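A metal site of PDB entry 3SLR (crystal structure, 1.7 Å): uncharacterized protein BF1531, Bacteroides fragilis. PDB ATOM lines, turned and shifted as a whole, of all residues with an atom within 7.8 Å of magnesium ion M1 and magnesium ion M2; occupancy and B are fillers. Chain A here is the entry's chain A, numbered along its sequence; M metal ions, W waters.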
ATOM      1  N   LEU A 227     -12.079  -4.901   0.043  1.00  0.00           N
ATOM      2  CA  LEU A 227     -11.524  -5.636   1.174  1.00  0.00           C
ATOM      3  C   LEU A 227     -12.202  -6.986   1.391  1.00  0.00           C
ATOM      4  O   LEU A 227     -13.413  -7.080   1.438  1.00  0.00           O
ATOM      5  CB  LEU A 227     -11.685  -4.826   2.458  1.00  0.00           C
ATOM      6  CG  LEU A 227     -10.982  -3.469   2.471  1.00  0.00           C
ATOM      7  CD1 LEU A 227     -11.543  -2.580   3.591  1.00  0.00           C
ATOM      8  CD2 LEU A 227      -9.472  -3.648   2.593  1.00  0.00           C
ATOM      9  N   ASP A 228     -11.393  -8.029   1.564  1.00  0.00           N
ATOM     10  CA  ASP A 228     -11.890  -9.248   2.177  1.00  0.00           C
ATOM     11  C   ASP A 228     -12.089  -8.950   3.673  1.00  0.00           C
ATOM     12  O   ASP A 228     -11.588  -7.943   4.181  1.00  0.00           O
ATOM     13  CB  ASP A 228     -10.876 -10.363   1.955  1.00  0.00           C
ATOM     14  CG  ASP A 228     -11.214 -11.617   2.727  1.00  0.00           C
ATOM     15  OD1 ASP A 228     -12.272 -12.221   2.435  1.00  0.00           O
ATOM     16  OD2 ASP A 228     -10.422 -11.991   3.612  1.00  0.00           O
ATOM     17  N   LEU A 229     -12.838  -9.788   4.389  1.00  0.00           N
ATOM     18  CA  LEU A 229     -13.051  -9.563   5.813  1.00  0.00           C
ATOM     19  C   LEU A 229     -12.187 -10.473   6.682  1.00  0.00           C
ATOM     20  O   LEU A 229     -11.238 -10.016   7.335  1.00  0.00           O
ATOM     21  CB  LEU A 229     -14.535  -9.718   6.176  1.00  0.00           C
ATOM     22  CG  LEU A 229     -15.513  -8.710   5.549  1.00  0.00           C
ATOM     23  CD1 LEU A 229     -16.972  -9.049   5.920  1.00  0.00           C
ATOM     24  CD2 LEU A 229     -15.169  -7.270   5.948  1.00  0.00           C
ATOM     25  N   ASP A 230     -12.483 -11.766   6.688  1.00  0.00           N
ATOM     26  CA  ASP A 230     -11.801 -12.682   7.622  1.00  0.00           C
ATOM     27  C   ASP A 230     -10.286 -12.712   7.417  1.00  0.00           C
ATOM     28  O   ASP A 230      -9.797 -13.033   6.326  1.00  0.00           O
ATOM     29  CB  ASP A 230     -12.385 -14.097   7.530  1.00  0.00           C
ATOM     30  CG  ASP A 230     -13.799 -14.204   8.078  1.00  0.00           C
ATOM     31  OD1 ASP A 230     -14.147 -13.528   9.088  1.00  0.00           O
ATOM     32  OD2 ASP A 230     -14.578 -14.992   7.508  1.00  0.00           O
ATOM     33  N   ASN A 231      -9.548 -12.398   8.475  1.00  0.00           N
ATOM     34  CA  ASN A 231      -8.099 -12.403   8.432  1.00  0.00           C
ATOM     35  C   ASN A 231      -7.504 -11.353   7.495  1.00  0.00           C
ATOM     36  O   ASN A 231      -6.322 -11.382   7.193  1.00  0.00           O
ATOM     37  CB  ASN A 231      -7.547 -13.800   8.147  1.00  0.00           C
ATOM     38  CG  ASN A 231      -7.798 -14.752   9.306  1.00  0.00           C
ATOM     39  OD1 ASN A 231      -7.604 -14.404  10.479  1.00  0.00           O
ATOM     40  ND2 ASN A 231      -8.257 -15.964   8.985  1.00  0.00           N
ATOM     41  N   THR A 232      -8.339 -10.411   7.067  1.00  0.00           N
ATOM     42  CA  THR A 232      -7.877  -9.264   6.304  1.00  0.00           C
ATOM     43  C   THR A 232      -8.057  -7.990   7.108  1.00  0.00           C
ATOM     44  O   THR A 232      -7.061  -7.302   7.402  1.00  0.00           O
ATOM     45  CB  THR A 232      -8.569  -9.189   4.906  1.00  0.00           C
ATOM     46  OG1 THR A 232      -8.218 -10.355   4.154  1.00  0.00           O
ATOM     47  CG2 THR A 232      -8.079  -7.977   4.122  1.00  0.00           C
ATOM     48  N   ILE A 233      -9.279  -7.689   7.530  1.00  0.00           N
ATOM     49  CA  ILE A 233      -9.494  -6.530   8.414  1.00  0.00           C
ATOM     50  C   ILE A 233      -9.716  -6.887   9.901  1.00  0.00           C
ATOM     51  O   ILE A 233      -9.784  -6.003  10.742  1.00  0.00           O
ATOM     52  CB  ILE A 233     -10.598  -5.578   7.912  1.00  0.00           C
ATOM     53  CG1 ILE A 233     -11.994  -6.202   8.049  1.00  0.00           C
ATOM     54  CG2 ILE A 233     -10.300  -5.147   6.479  1.00  0.00           C
ATOM     55  CD1 ILE A 233     -13.122  -5.193   7.967  1.00  0.00           C
ATOM     56  N   TRP A 234      -9.865  -8.168  10.201  1.00  0.00           N
ATOM     57  CA  TRP A 234      -9.886  -8.639  11.595  1.00  0.00           C
ATOM     58  C   TRP A 234      -9.290 -10.029  11.628  1.00  0.00           C
ATOM     59  O   TRP A 234      -9.258 -10.718  10.610  1.00  0.00           O
ATOM     60  CB  TRP A 234     -11.312  -8.638  12.201  1.00  0.00           C
ATOM     61  CG  TRP A 234     -12.349  -9.500  11.469  1.00  0.00           C
ATOM     62  CD1 TRP A 234     -12.293 -10.840  11.234  1.00  0.00           C
ATOM     63  CD2 TRP A 234     -13.602  -9.042  10.923  1.00  0.00           C
ATOM     64  NE1 TRP A 234     -13.424 -11.250  10.548  1.00  0.00           N
ATOM     65  CE2 TRP A 234     -14.241 -10.164  10.347  1.00  0.00           C
ATOM     66  CE3 TRP A 234     -14.237  -7.799  10.847  1.00  0.00           C
ATOM     67  CZ2 TRP A 234     -15.489 -10.079   9.711  1.00  0.00           C
ATOM     68  CZ3 TRP A 234     -15.474  -7.710  10.220  1.00  0.00           C
ATOM     69  CH2 TRP A 234     -16.085  -8.846   9.660  1.00  0.00           C
ATOM     70  N   GLY A 236      -9.243 -13.973  12.589  1.00  0.00           N
ATOM     71  CA  GLY A 236     -10.224 -15.005  12.832  1.00  0.00           C
ATOM     72  C   GLY A 236     -11.278 -15.097  11.757  1.00  0.00           C
ATOM     73  O   GLY A 236     -11.257 -14.337  10.781  1.00  0.00           O
ATOM     74  N   VAL A 237     -12.196 -16.027  11.935  1.00  0.00           N
ATOM     75  CA  VAL A 237     -13.228 -16.277  10.930  1.00  0.00           C
ATOM     76  C   VAL A 237     -14.568 -16.072  11.605  1.00  0.00           C
ATOM     77  O   VAL A 237     -14.924 -16.805  12.536  1.00  0.00           O
ATOM     78  CB  VAL A 237     -13.106 -17.700  10.369  1.00  0.00           C
ATOM     79  CG1 VAL A 237     -14.253 -18.004   9.397  1.00  0.00           C
ATOM     80  CG2 VAL A 237     -11.751 -17.865   9.663  1.00  0.00           C
ATOM     81  N   VAL A 238     -15.302 -15.062  11.157  1.00  0.00           N
ATOM     82  CA  VAL A 238     -16.490 -14.639  11.883  1.00  0.00           C
ATOM     83  C   VAL A 238     -17.552 -15.745  11.941  1.00  0.00           C
ATOM     84  O   VAL A 238     -18.254 -15.895  12.968  1.00  0.00           O
ATOM     85  CB  VAL A 238     -17.072 -13.311  11.330  1.00  0.00           C
ATOM     86  CG1 VAL A 238     -17.644 -13.490   9.913  1.00  0.00           C
ATOM     87  CG2 VAL A 238     -18.123 -12.755  12.266  1.00  0.00           C
ATOM     88  N   CYS A 278     -15.781  -7.493  -0.254  1.00  0.00           N
ATOM     89  CA  CYS A 278     -16.024  -8.667  -1.078  1.00  0.00           C
ATOM     90  C   CYS A 278     -15.578  -9.904  -0.310  1.00  0.00           C
ATOM     91  O   CYS A 278     -14.387 -10.173  -0.180  1.00  0.00           O
ATOM     92  CB  CYS A 278     -15.273  -8.576  -2.417  1.00  0.00           C
ATOM     93  SG  CYS A 278     -15.708  -9.922  -3.586  1.00  0.00           S
ATOM     94  N   SER A 279     -16.548 -10.631   0.229  1.00  0.00           N
ATOM     95  CA  SER A 279     -16.277 -11.663   1.223  1.00  0.00           C
ATOM     96  C   SER A 279     -17.092 -12.931   0.977  1.00  0.00           C
ATOM     97  O   SER A 279     -18.256 -12.858   0.561  1.00  0.00           O
ATOM     98  CB  SER A 279     -16.565 -11.089   2.613  1.00  0.00           C
ATOM     99  OG  SER A 279     -16.447 -12.071   3.640  1.00  0.00           O
ATOM    100  N   LYS A 280     -16.482 -14.081   1.212  1.00  0.00           N
ATOM    101  CA  LYS A 280     -17.165 -15.369   1.210  1.00  0.00           C
ATOM    102  C   LYS A 280     -17.801 -15.531   2.590  1.00  0.00           C
ATOM    103  O   LYS A 280     -17.154 -15.991   3.521  1.00  0.00           O
ATOM    104  CB  LYS A 280     -16.148 -16.494   0.987  1.00  0.00           C
ATOM    105  CG  LYS A 280     -16.384 -17.395  -0.217  1.00  0.00           C
ATOM    106  CD  LYS A 280     -16.358 -16.635  -1.517  1.00  0.00           C
ATOM    107  CE  LYS A 280     -16.110 -17.548  -2.737  1.00  0.00           C
ATOM    108  NZ  LYS A 280     -14.729 -18.116  -2.799  1.00  0.00           N
ATOM    109  N   ASN A 281     -19.067 -15.119   2.710  1.00  0.00           N
ATOM    110  CA  ASN A 281     -19.784 -15.149   3.977  1.00  0.00           C
ATOM    111  C   ASN A 281     -21.267 -14.929   3.753  1.00  0.00           C
ATOM    112  O   ASN A 281     -21.682 -14.369   2.735  1.00  0.00           O
ATOM    113  CB  ASN A 281     -19.278 -14.044   4.923  1.00  0.00           C
ATOM    114  CG  ASN A 281     -18.145 -14.495   5.840  1.00  0.00           C
ATOM    115  OD1 ASN A 281     -17.087 -13.847   5.901  1.00  0.00           O
ATOM    116  ND2 ASN A 281     -18.370 -15.567   6.575  1.00  0.00           N
ATOM    117  N   TRP A 310     -21.565 -16.478  -1.345  1.00  0.00           N
ATOM    118  CA  TRP A 310     -20.723 -17.667  -1.527  1.00  0.00           C
ATOM    119  C   TRP A 310     -20.300 -17.860  -2.977  1.00  0.00           C
ATOM    120  O   TRP A 310     -19.751 -18.897  -3.365  1.00  0.00           O
ATOM    121  CB  TRP A 310     -21.435 -18.902  -0.967  1.00  0.00           C
ATOM    122  CG  TRP A 310     -21.741 -18.734   0.497  1.00  0.00           C
ATOM    123  CD1 TRP A 310     -22.939 -18.395   1.059  1.00  0.00           C
ATOM    124  CD2 TRP A 310     -20.811 -18.856   1.588  1.00  0.00           C
ATOM    125  NE1 TRP A 310     -22.812 -18.302   2.430  1.00  0.00           N
ATOM    126  CE2 TRP A 310     -21.516 -18.587   2.777  1.00  0.00           C
ATOM    127  CE3 TRP A 310     -19.450 -19.169   1.673  1.00  0.00           C
ATOM    128  CZ2 TRP A 310     -20.913 -18.638   4.037  1.00  0.00           C
ATOM    129  CZ3 TRP A 310     -18.852 -19.209   2.924  1.00  0.00           C
ATOM    130  CH2 TRP A 310     -19.579 -18.946   4.085  1.00  0.00           C
ATOM    131  N   LYS A 313     -15.296 -14.541  -6.233  1.00  0.00           N
ATOM    132  CA  LYS A 313     -15.065 -13.120  -6.033  1.00  0.00           C
ATOM    133  C   LYS A 313     -14.922 -12.338  -7.357  1.00  0.00           C
ATOM    134  O   LYS A 313     -15.244 -11.158  -7.417  1.00  0.00           O
ATOM    135  CB  LYS A 313     -13.871 -12.901  -5.112  1.00  0.00           C
ATOM    136  CG  LYS A 313     -14.132 -13.485  -3.731  1.00  0.00           C
ATOM    137  CD  LYS A 313     -13.137 -12.973  -2.708  1.00  0.00           C
ATOM    138  CE  LYS A 313     -13.540 -13.426  -1.323  1.00  0.00           C
ATOM    139  NZ  LYS A 313     -12.890 -12.600  -0.268  1.00  0.00           N
ATOM    140  N   LEU A 334      -7.685  -6.371  -1.681  1.00  0.00           N
ATOM    141  CA  LEU A 334      -6.888  -6.963  -0.605  1.00  0.00           C
ATOM    142  C   LEU A 334      -7.552  -8.197  -0.001  1.00  0.00           C
ATOM    143  O   LEU A 334      -8.673  -8.123   0.507  1.00  0.00           O
ATOM    144  CB  LEU A 334      -6.633  -5.940   0.502  1.00  0.00           C
ATOM    145  CG  LEU A 334      -5.849  -4.683   0.085  1.00  0.00           C
ATOM    146  CD1 LEU A 334      -5.723  -3.745   1.286  1.00  0.00           C
ATOM    147  CD2 LEU A 334      -4.482  -5.062  -0.440  1.00  0.00           C
ATOM    148  N   ASP A 335      -6.844  -9.328  -0.051  1.00  0.00           N
ATOM    149  CA  ASP A 335      -7.357 -10.604   0.430  1.00  0.00           C
ATOM    150  C   ASP A 335      -6.193 -11.451   0.949  1.00  0.00           C
ATOM    151  O   ASP A 335      -5.163 -11.562   0.280  1.00  0.00           O
ATOM    152  CB  ASP A 335      -8.119 -11.323  -0.695  1.00  0.00           C
ATOM    153  CG  ASP A 335      -8.990 -12.458  -0.199  1.00  0.00           C
ATOM    154  OD1 ASP A 335      -8.525 -13.240   0.659  1.00  0.00           O
ATOM    155  OD2 ASP A 335     -10.149 -12.569  -0.676  1.00  0.00           O
ATOM    156  N   ASP A 336      -6.326 -12.005   2.142  1.00  0.00           N
ATOM    157  CA  ASP A 336      -5.259 -12.780   2.779  1.00  0.00           C
ATOM    158  C   ASP A 336      -5.086 -14.158   2.142  1.00  0.00           C
ATOM    159  O   ASP A 336      -4.092 -14.834   2.369  1.00  0.00           O
ATOM    160  CB  ASP A 336      -5.564 -12.964   4.265  1.00  0.00           C
ATOM    161  CG  ASP A 336      -6.740 -13.880   4.479  1.00  0.00           C
ATOM    162  OD1 ASP A 336      -7.843 -13.460   4.092  1.00  0.00           O
ATOM    163  OD2 ASP A 336      -6.583 -15.022   4.978  1.00  0.00           O
ATOM    164  N   ASN A 337      -6.072 -14.583   1.364  1.00  0.00           N
ATOM    165  CA  ASN A 337      -6.051 -15.920   0.750  1.00  0.00           C
ATOM    166  C   ASN A 337      -5.411 -15.894  -0.648  1.00  0.00           C
ATOM    167  O   ASN A 337      -5.958 -15.254  -1.543  1.00  0.00           O
ATOM    168  CB  ASN A 337      -7.492 -16.439   0.635  1.00  0.00           C
ATOM    169  CG  ASN A 337      -7.549 -17.899   0.248  1.00  0.00           C
ATOM    170  OD1 ASN A 337      -6.809 -18.368  -0.612  1.00  0.00           O
ATOM    171  ND2 ASN A 337      -8.458 -18.647   0.889  1.00  0.00           N
ATOM    172  N   GLU A 340      -7.729 -16.773  -3.612  1.00  0.00           N
ATOM    173  CA  GLU A 340      -8.631 -15.673  -3.942  1.00  0.00           C
ATOM    174  C   GLU A 340      -7.894 -14.587  -4.735  1.00  0.00           C
ATOM    175  O   GLU A 340      -8.398 -14.110  -5.765  1.00  0.00           O
ATOM    176  CB  GLU A 340      -9.267 -15.068  -2.685  1.00  0.00           C
ATOM    177  CG  GLU A 340     -10.158 -16.008  -1.854  1.00  0.00           C
ATOM    178  CD  GLU A 340     -11.481 -16.358  -2.542  1.00  0.00           C
ATOM    179  OE1 GLU A 340     -11.634 -16.052  -3.739  1.00  0.00           O
ATOM    180  OE2 GLU A 340     -12.370 -16.942  -1.876  1.00  0.00           O
ATOM    181  N   TYR A 363       1.298  -6.461   7.089  1.00  0.00           N
ATOM    182  CA  TYR A 363       0.474  -5.981   5.980  1.00  0.00           C
ATOM    183  C   TYR A 363       0.786  -4.513   5.647  1.00  0.00           C
ATOM    184  O   TYR A 363       1.028  -4.160   4.501  1.00  0.00           O
ATOM    185  CB  TYR A 363      -1.016  -6.040   6.309  1.00  0.00           C
ATOM    186  CG  TYR A 363      -1.662  -7.409   6.288  1.00  0.00           C
ATOM    187  CD1 TYR A 363      -0.960  -8.542   5.905  1.00  0.00           C
ATOM    188  CD2 TYR A 363      -3.006  -7.559   6.663  1.00  0.00           C
ATOM    189  CE1 TYR A 363      -1.580  -9.797   5.896  1.00  0.00           C
ATOM    190  CE2 TYR A 363      -3.623  -8.793   6.665  1.00  0.00           C
ATOM    191  CZ  TYR A 363      -2.909  -9.901   6.282  1.00  0.00           C
ATOM    192  OH  TYR A 363      -3.536 -11.137   6.275  1.00  0.00           O
HETATM  193 MG    MG M   1      -9.849 -14.042   4.252  1.00  0.00          MG
HETATM  194 MG    MG M   2     -13.393 -13.954   3.723  1.00  0.00          MG
HETATM  195  O   HOH W   1      -8.882 -16.179   4.987  1.00  0.00           O
HETATM  196  O   HOH W   2     -11.659 -15.285   4.252  1.00  0.00           O
HETATM  197  O   HOH W   3     -14.339 -15.751   4.761  1.00  0.00           O
HETATM  198  O   HOH W   4     -13.626 -14.501   1.606  1.00  0.00           O
HETATM  199  O   HOH W   5     -14.322 -12.485   4.556  1.00  0.00           O
HETATM  200  O   HOH W   6     -10.030 -14.781   1.998  1.00  0.00           O
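Asp 335 touches magnesium ion M1. Of the 23 residues printed, 4 come within 4 Å of magnesium ion M1. The nearest printed residue that does not touch magnesium ion M1 is Thr 232 (4.03 Å).
Residues that only touch magnesium ion M2: Ser 279 (3.6 Å) and Lys 280 (3.98 Å). Within 4 Å of magnesium ion M2: Asp 228, Asp 230, Ser 279 and Lys 280.
Magnesium ion M1 is bound by OD1 of Asp 336 (2.1 Å), water W2 (2.2 Å), OD2 of Asp 228 (2.2 Å), O of Asp 230 (2.3 Å), water W6 (2.4 Å) and water W1 (2.5 Å).
Water W3 bridges OD2 of Asp 230 and O of Lys 280. Water W4 lies within hydrogen-bond range of the side-chain amino group of Lys 313 (2.8 Å) and the backbone NH of Lys 280 (2.9 Å). Water W5 lies within hydrogen-bond range of N of Asp 230 (2.9 Å), N of Leu 229 (3.1 Å) and OD1 of Asn 281 (3.4 Å).
OD2 of Asp 230 sits close to OD1 of Asn 281 (3.2 Å). The side-chain carboxylate (OD1) of Asp 230 is in hydrogen-bond range of the indole nitrogen (NE1) of Trp 234 (2.8 Å). OD2 of Asp 335 lies within salt-bridge range of NZ of Lys 313 (2.8 Å). The side-chain carboxylate (OD1) of Asp 228 sits close to the side-chain amino group (NZ) of Lys 313 (2.8 Å). N of Asp 336 lies within hydrogen-bond range of OG1 of Thr 232 (3.2 Å). The side-chain carboxylate (OD1) of Asp 335 is in hydrogen-bond range of the backbone NH (N) of Asn 337, at 2.9 Å. OD2 of Asp 228 sits close to OG1 of Thr 232. OD1 of Asp 230 lies within hydrogen-bond range of N of Val 238.
Magnesium ion M2 is bound by water W5 (1.9 Å), water W4 (2.2 Å), water W2 (2.2 Å), water W3 (2.3 Å) and the side-chain carboxylate of Asp 228 (2.4 Å).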
